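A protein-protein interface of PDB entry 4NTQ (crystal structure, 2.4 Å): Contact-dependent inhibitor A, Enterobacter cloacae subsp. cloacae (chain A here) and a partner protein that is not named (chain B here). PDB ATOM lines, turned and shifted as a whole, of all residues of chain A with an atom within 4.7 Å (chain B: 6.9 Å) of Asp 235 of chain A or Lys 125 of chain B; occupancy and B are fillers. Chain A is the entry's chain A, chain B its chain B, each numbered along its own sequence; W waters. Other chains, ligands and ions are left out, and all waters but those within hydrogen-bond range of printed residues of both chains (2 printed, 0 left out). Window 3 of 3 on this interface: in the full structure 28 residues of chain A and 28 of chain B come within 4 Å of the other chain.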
ATOM      1  N   ARG A 222       7.018  14.013 -10.146  1.00  0.00           N
ATOM      2  CA  ARG A 222       5.642  13.669  -9.788  1.00  0.00           C
ATOM      3  C   ARG A 222       5.577  12.254  -9.249  1.00  0.00           C
ATOM      4  O   ARG A 222       6.063  11.312  -9.888  1.00  0.00           O
ATOM      5  CB  ARG A 222       4.734  13.779 -10.999  1.00  0.00           C
ATOM      6  CG  ARG A 222       3.253  13.543 -10.727  1.00  0.00           C
ATOM      7  CD  ARG A 222       2.428  14.059 -11.911  1.00  0.00           C
ATOM      8  NE  ARG A 222       1.066  13.532 -11.950  1.00  0.00           N
ATOM      9  CZ  ARG A 222       0.142  13.920 -12.831  1.00  0.00           C
ATOM     10  NH1 ARG A 222       0.438  14.848 -13.741  1.00  0.00           N
ATOM     11  NH2 ARG A 222      -1.076  13.381 -12.804  1.00  0.00           N
ATOM     12  N   ILE A 223       4.985  12.103  -8.071  1.00  0.00           N
ATOM     13  CA  ILE A 223       4.868  10.780  -7.463  1.00  0.00           C
ATOM     14  C   ILE A 223       3.424  10.423  -7.156  1.00  0.00           C
ATOM     15  O   ILE A 223       3.147   9.622  -6.255  1.00  0.00           O
ATOM     16  CB  ILE A 223       5.751  10.612  -6.209  1.00  0.00           C
ATOM     17  CG1 ILE A 223       5.498  11.736  -5.207  1.00  0.00           C
ATOM     18  CG2 ILE A 223       7.220  10.554  -6.597  1.00  0.00           C
ATOM     19  CD1 ILE A 223       6.195  11.510  -3.846  1.00  0.00           C
ATOM     20  N   GLY A 224       2.509  11.037  -7.907  1.00  0.00           N
ATOM     21  CA  GLY A 224       1.131  10.583  -7.940  1.00  0.00           C
ATOM     22  C   GLY A 224       0.016  11.615  -7.879  1.00  0.00           C
ATOM     23  O   GLY A 224       0.212  12.772  -7.494  1.00  0.00           O
ATOM     24  N   THR A 225      -1.175  11.174  -8.271  1.00  0.00           N
ATOM     25  CA  THR A 225      -2.389  11.941  -8.052  1.00  0.00           C
ATOM     26  C   THR A 225      -2.980  11.429  -6.748  1.00  0.00           C
ATOM     27  O   THR A 225      -2.991  10.230  -6.531  1.00  0.00           O
ATOM     28  CB  THR A 225      -3.383  11.723  -9.191  1.00  0.00           C
ATOM     29  OG1 THR A 225      -2.880  12.336 -10.388  1.00  0.00           O
ATOM     30  CG2 THR A 225      -4.735  12.334  -8.834  1.00  0.00           C
ATOM     31  N   ARG A 232      -2.926   7.862  -2.409  1.00  0.00           N
ATOM     32  CA  ARG A 232      -2.599   7.755  -3.820  1.00  0.00           C
ATOM     33  C   ARG A 232      -3.721   7.093  -4.589  1.00  0.00           C
ATOM     34  O   ARG A 232      -4.240   6.056  -4.182  1.00  0.00           O
ATOM     35  CB  ARG A 232      -1.321   6.931  -3.993  1.00  0.00           C
ATOM     36  CG  ARG A 232      -0.622   7.131  -5.317  1.00  0.00           C
ATOM     37  CD  ARG A 232       0.525   6.146  -5.480  1.00  0.00           C
ATOM     38  NE  ARG A 232       1.339   6.466  -6.641  1.00  0.00           N
ATOM     39  CZ  ARG A 232       1.015   6.134  -7.886  1.00  0.00           C
ATOM     40  NH1 ARG A 232      -0.103   5.473  -8.127  1.00  0.00           N
ATOM     41  NH2 ARG A 232       1.809   6.470  -8.891  1.00  0.00           N
ATOM     42  N   LYS A 234      -3.709   7.269  -8.415  1.00  0.00           N
ATOM     43  CA  LYS A 234      -3.124   6.862  -9.681  1.00  0.00           C
ATOM     44  C   LYS A 234      -1.904   7.737  -9.933  1.00  0.00           C
ATOM     45  O   LYS A 234      -1.506   8.526  -9.072  1.00  0.00           O
ATOM     46  CB  LYS A 234      -4.134   7.056 -10.809  1.00  0.00           C
ATOM     47  CG  LYS A 234      -4.567   8.500 -10.971  1.00  0.00           C
ATOM     48  CD  LYS A 234      -5.789   8.652 -11.872  1.00  0.00           C
ATOM     49  CE  LYS A 234      -6.178  10.123 -12.010  1.00  0.00           C
ATOM     50  NZ  LYS A 234      -7.476  10.328 -12.732  1.00  0.00           N
ATOM     51  N   ASP A 235      -1.314   7.606 -11.112  1.00  0.00           N
ATOM     52  CA  ASP A 235      -0.187   8.455 -11.479  1.00  0.00           C
ATOM     53  C   ASP A 235      -0.613   9.927 -11.507  1.00  0.00           C
ATOM     54  O   ASP A 235       0.229  10.798 -11.322  1.00  0.00           O
ATOM     55  CB  ASP A 235       0.391   8.031 -12.835  1.00  0.00           C
ATOM     56  CG  ASP A 235       1.265   6.796 -12.736  1.00  0.00           C
ATOM     57  OD1 ASP A 235       1.075   6.008 -11.782  1.00  0.00           O
ATOM     58  OD2 ASP A 235       2.149   6.621 -13.608  1.00  0.00           O
ATOM     59  N   TYR B  28      -3.997   9.073 -22.445  1.00  0.00           N
ATOM     60  CA  TYR B  28      -4.048   9.971 -21.301  1.00  0.00           C
ATOM     61  C   TYR B  28      -4.182  11.436 -21.728  1.00  0.00           C
ATOM     62  O   TYR B  28      -3.559  11.880 -22.701  1.00  0.00           O
ATOM     63  CB  TYR B  28      -2.819   9.780 -20.412  1.00  0.00           C
ATOM     64  CG  TYR B  28      -2.775  10.676 -19.189  1.00  0.00           C
ATOM     65  CD1 TYR B  28      -3.473  10.337 -18.027  1.00  0.00           C
ATOM     66  CD2 TYR B  28      -2.028  11.863 -19.190  1.00  0.00           C
ATOM     67  CE1 TYR B  28      -3.430  11.155 -16.894  1.00  0.00           C
ATOM     68  CE2 TYR B  28      -1.979  12.683 -18.060  1.00  0.00           C
ATOM     69  CZ  TYR B  28      -2.689  12.326 -16.920  1.00  0.00           C
ATOM     70  OH  TYR B  28      -2.647  13.133 -15.797  1.00  0.00           O
ATOM     71  N   GLU B  30      -4.758  15.539 -19.676  1.00  0.00           N
ATOM     72  CA  GLU B  30      -4.797  16.254 -18.409  1.00  0.00           C
ATOM     73  C   GLU B  30      -4.901  17.724 -18.708  1.00  0.00           C
ATOM     74  O   GLU B  30      -4.151  18.227 -19.539  1.00  0.00           O
ATOM     75  CB  GLU B  30      -3.521  15.997 -17.593  1.00  0.00           C
ATOM     76  CG  GLU B  30      -3.426  16.850 -16.325  1.00  0.00           C
ATOM     77  CD  GLU B  30      -2.227  16.500 -15.450  1.00  0.00           C
ATOM     78  OE1 GLU B  30      -1.811  15.324 -15.442  1.00  0.00           O
ATOM     79  OE2 GLU B  30      -1.708  17.403 -14.762  1.00  0.00           O
ATOM     80  N   ASN B  93       6.176  14.216 -15.561  1.00  0.00           N
ATOM     81  CA  ASN B  93       5.676  15.542 -15.260  1.00  0.00           C
ATOM     82  C   ASN B  93       6.492  16.009 -14.085  1.00  0.00           C
ATOM     83  O   ASN B  93       6.340  15.500 -12.974  1.00  0.00           O
ATOM     84  CB  ASN B  93       4.173  15.453 -14.920  1.00  0.00           C
ATOM     85  CG  ASN B  93       3.573  16.782 -14.449  1.00  0.00           C
ATOM     86  OD1 ASN B  93       2.667  16.788 -13.605  1.00  0.00           O
ATOM     87  ND2 ASN B  93       4.062  17.908 -14.997  1.00  0.00           N
ATOM     88  N   THR B 118      12.769   5.770 -12.816  1.00  0.00           N
ATOM     89  CA  THR B 118      11.425   5.254 -12.612  1.00  0.00           C
ATOM     90  C   THR B 118      10.951   5.213 -11.144  1.00  0.00           C
ATOM     91  O   THR B 118       9.753   5.117 -10.887  1.00  0.00           O
ATOM     92  CB  THR B 118      11.281   3.866 -13.241  1.00  0.00           C
ATOM     93  OG1 THR B 118      12.252   2.989 -12.663  1.00  0.00           O
ATOM     94  CG2 THR B 118      11.492   3.956 -14.751  1.00  0.00           C
ATOM     95  N   HIS B 119      11.878   5.278 -10.193  1.00  0.00           N
ATOM     96  CA  HIS B 119      11.526   5.331  -8.768  1.00  0.00           C
ATOM     97  C   HIS B 119      12.522   6.250  -8.068  1.00  0.00           C
ATOM     98  O   HIS B 119      13.673   6.320  -8.482  1.00  0.00           O
ATOM     99  CB  HIS B 119      11.555   3.930  -8.120  1.00  0.00           C
ATOM    100  CG  HIS B 119      10.843   2.872  -8.913  1.00  0.00           C
ATOM    101  ND1 HIS B 119      11.455   2.162  -9.927  1.00  0.00           N
ATOM    102  CD2 HIS B 119       9.573   2.406  -8.842  1.00  0.00           C
ATOM    103  CE1 HIS B 119      10.591   1.304 -10.446  1.00  0.00           C
ATOM    104  NE2 HIS B 119       9.443   1.430  -9.804  1.00  0.00           N
ATOM    105  N   ASP B 120      12.099   6.963  -7.025  1.00  0.00           N
ATOM    106  CA  ASP B 120      13.030   7.840  -6.317  1.00  0.00           C
ATOM    107  C   ASP B 120      13.784   7.097  -5.226  1.00  0.00           C
ATOM    108  O   ASP B 120      13.655   5.880  -5.085  1.00  0.00           O
ATOM    109  CB  ASP B 120      12.377   9.128  -5.783  1.00  0.00           C
ATOM    110  CG  ASP B 120      11.230   8.880  -4.793  1.00  0.00           C
ATOM    111  OD1 ASP B 120      10.358   9.769  -4.697  1.00  0.00           O
ATOM    112  OD2 ASP B 120      11.180   7.838  -4.110  1.00  0.00           O
ATOM    113  N   GLY B 123      11.846   4.950  -2.968  1.00  0.00           N
ATOM    114  CA  GLY B 123      11.118   3.851  -3.572  1.00  0.00           C
ATOM    115  C   GLY B 123       9.768   4.199  -4.181  1.00  0.00           C
ATOM    116  O   GLY B 123       9.023   3.308  -4.587  1.00  0.00           O
ATOM    117  N   MET B 124       9.435   5.486  -4.243  1.00  0.00           N
ATOM    118  CA  MET B 124       8.139   5.892  -4.776  1.00  0.00           C
ATOM    119  C   MET B 124       8.154   5.874  -6.302  1.00  0.00           C
ATOM    120  O   MET B 124       9.115   6.331  -6.925  1.00  0.00           O
ATOM    121  CB  MET B 124       7.767   7.283  -4.269  1.00  0.00           C
ATOM    122  CG  MET B 124       7.453   7.331  -2.789  1.00  0.00           C
ATOM    123  SD  MET B 124       5.778   6.399  -2.434  1.00  0.00           S
ATOM    124  CE  MET B 124       4.570   7.654  -3.336  1.00  0.00           C
ATOM    125  N   LYS B 125       7.104   5.326  -6.905  1.00  0.00           N
ATOM    126  CA  LYS B 125       7.027   5.305  -8.354  1.00  0.00           C
ATOM    127  C   LYS B 125       6.960   6.728  -8.897  1.00  0.00           C
ATOM    128  O   LYS B 125       6.175   7.547  -8.429  1.00  0.00           O
ATOM    129  CB  LYS B 125       5.833   4.491  -8.839  1.00  0.00           C
ATOM    130  CG  LYS B 125       5.615   4.596 -10.339  1.00  0.00           C
ATOM    131  CD  LYS B 125       4.327   3.924 -10.762  1.00  0.00           C
ATOM    132  CE  LYS B 125       4.016   4.205 -12.223  1.00  0.00           C
ATOM    133  NZ  LYS B 125       2.932   3.316 -12.707  1.00  0.00           N
ATOM    134  N   ILE B 126       7.821   7.026  -9.860  1.00  0.00           N
ATOM    135  CA  ILE B 126       7.739   8.289 -10.570  1.00  0.00           C
ATOM    136  C   ILE B 126       6.599   8.157 -11.570  1.00  0.00           C
ATOM    137  O   ILE B 126       6.515   7.164 -12.289  1.00  0.00           O
ATOM    138  CB  ILE B 126       9.036   8.588 -11.327  1.00  0.00           C
ATOM    139  CG1 ILE B 126      10.234   8.527 -10.369  1.00  0.00           C
ATOM    140  CG2 ILE B 126       8.950   9.939 -12.043  1.00  0.00           C
ATOM    141  CD1 ILE B 126      10.246   9.641  -9.399  1.00  0.00           C
ATOM    142  N   SER B 127       5.705   9.136 -11.598  1.00  0.00           N
ATOM    143  CA  SER B 127       4.610   9.085 -12.551  1.00  0.00           C
ATOM    144  C   SER B 127       5.171   9.093 -13.973  1.00  0.00           C
ATOM    145  O   SER B 127       6.104   9.827 -14.274  1.00  0.00           O
ATOM    146  CB  SER B 127       3.650  10.253 -12.333  1.00  0.00           C
ATOM    147  OG  SER B 127       2.951  10.154 -11.098  1.00  0.00           O
ATOM    148  N   GLU B 128       4.608   8.264 -14.842  1.00  0.00           N
ATOM    149  CA  GLU B 128       5.119   8.128 -16.203  1.00  0.00           C
ATOM    150  C   GLU B 128       4.043   7.651 -17.185  1.00  0.00           C
ATOM    151  O   GLU B 128       3.220   6.795 -16.866  1.00  0.00           O
ATOM    152  CB  GLU B 128       6.313   7.161 -16.224  1.00  0.00           C
ATOM    153  CG  GLU B 128       7.089   7.161 -17.530  1.00  0.00           C
ATOM    154  CD  GLU B 128       8.344   6.293 -17.471  1.00  0.00           C
ATOM    155  OE1 GLU B 128       8.215   5.053 -17.527  1.00  0.00           O
ATOM    156  OE2 GLU B 128       9.455   6.854 -17.376  1.00  0.00           O
ATOM    157  N   TRP B 129       4.059   8.202 -18.387  1.00  0.00           N
ATOM    158  CA  TRP B 129       3.138   7.764 -19.427  1.00  0.00           C
ATOM    159  C   TRP B 129       3.966   7.474 -20.679  1.00  0.00           C
ATOM    160  O   TRP B 129       5.148   7.819 -20.739  1.00  0.00           O
ATOM    161  CB  TRP B 129       2.105   8.865 -19.714  1.00  0.00           C
ATOM    162  CG  TRP B 129       1.202   9.218 -18.539  1.00  0.00           C
ATOM    163  CD1 TRP B 129      -0.097   8.827 -18.361  1.00  0.00           C
ATOM    164  CD2 TRP B 129       1.528  10.040 -17.405  1.00  0.00           C
ATOM    165  NE1 TRP B 129      -0.595   9.343 -17.186  1.00  0.00           N
ATOM    166  CE2 TRP B 129       0.378  10.097 -16.585  1.00  0.00           C
ATOM    167  CE3 TRP B 129       2.671  10.732 -17.007  1.00  0.00           C
ATOM    168  CZ2 TRP B 129       0.343  10.818 -15.385  1.00  0.00           C
ATOM    169  CZ3 TRP B 129       2.640  11.442 -15.808  1.00  0.00           C
ATOM    170  CH2 TRP B 129       1.479  11.485 -15.015  1.00  0.00           C
HETATM  171  O   HOH W   1       3.511   8.217  -9.282  1.00  0.00           O
HETATM  172  O   HOH W   2       3.286   3.980 -15.514  1.00  0.00           O
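NZ of Lys 125 of chain B lies within salt-bridge range of OD1 of Asp 235 of chain A, at 3.4 Å.
N of Glu 128 of chain B lies within hydrogen-bond range of OD2 of Asp 235 of chain A.
The side-chain hydroxyl of Ser 127 of chain B lies within hydrogen-bond range of the backbone NH of Gly 224 of chain A.
The guanidinium group of Arg 222 of chain A lies within hydrogen-bond range of the side-chain hydroxyl of Tyr 28 of chain B, at 3.4 Å.
OG of Ser 127 of chain B sits at hydrogen-bond distance from O of Asp 235 of chain A (2.8 Å).
The guanidinium group (NH1) of Arg 222 of chain A lies within salt-bridge range of the side-chain carboxylate (OE1) of Glu 30 of chain B, at 2.9 Å.
The guanidinium group (NH1) of Arg 222 of chain A is in hydrogen-bond range of the side-chain amide oxygen (OD1) of Asn 93 of chain B, 3.0 Å away.
The backbone carbonyl oxygen (O) of Arg 222 of chain A sits at hydrogen-bond distance from the backbone NH (N) of Ser 127 of chain B.
The guanidinium group (NH2) of Arg 222 of chain A is in hydrogen-bond range of the side-chain hydroxyl (OG1) of Thr 225 of chain A (3.2 Å).
O of Asp 235 of chain A sits at hydrogen-bond distance from NE of Arg 222 of chain A, 2.9 Å away.
The backbone NH (N) of Thr 225 of chain A lies within hydrogen-bond range of the backbone carbonyl oxygen (O) of Asp 235 of chain A, at 3.4 Å.
The side-chain carboxylate (OD1) of Asp 235 of chain A lies within salt-bridge range of the guanidinium group (NH2) of Arg 232 of chain A, at 3.0 Å.
OD2 of Asp 120 of chain B lies within hydrogen-bond range of N of Gly 123 of chain B.
O of Thr 118 of chain B sits at hydrogen-bond distance from N of Ile 126 of chain B.
Among the printed residues, pairs that only touch across the chains: Arg 222 of chain A with Ile 126 of chain B (3.5 Å), Arg 222 of chain A with Trp 129 of chain B (3.5 Å), Ile 223 of chain A with Asp 120 of chain B (3.8 Å), Ile 223 of chain A with Met 124 of chain B (3.8 Å), Ile 223 of chain A with Lys 125 of chain B (3.6 Å), Ile 223 of chain A with Ser 127 of chain B (3.98 Å) and Asp 235 of chain A with Trp 129 of chain B (3.8 Å).
Of chain B, only Lys 125, Ser 127, Glu 128 and Trp 129 come within 4 Å of Asp 235 of chain A.
Of the printed residues of chain A, Glu 128 of chain B touches Asp 235.
Of the printed residues of chain A, Ile 126 of chain B touches Arg 222.
Hydrophobic or aromatic side chains of chain A that line the printed part of chain B: Ile 223.
Of the 13 printed residues of chain B, 10 touch a printed residue of chain A.
Among the printed residues, 15 pairs touch across the chains.
Among the printed residues, Asp or Glu carboxylates within 4 Å of a Lys or Arg side-chain nitrogen of the other chain: Arg 222 of chain A with Glu 30 of chain B (2.9 Å) and Asp 235 of chain A with Lys 125 of chain B (3.4 Å).
Water W1 lies within hydrogen-bond range of the guanidinium group (NH2) of Arg 232 of chain A (2.5 Å), the side-chain hydroxyl (OG) of Ser 127 of chain B (2.7 Å), the backbone carbonyl oxygen (O) of Lys 125 of chain B (2.9 Å), the backbone NH (N) of Gly 224 of chain A (3.3 Å) and the backbone carbonyl oxygen (O) of Ile 223 of chain A (3.4 Å).
Water W2 lies within hydrogen-bond range of NZ of Lys 125 of chain B (2.9 Å), O of Glu 128 of chain B (3.1 Å) and OD2 of Asp 235 of chain A (3.4 Å).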
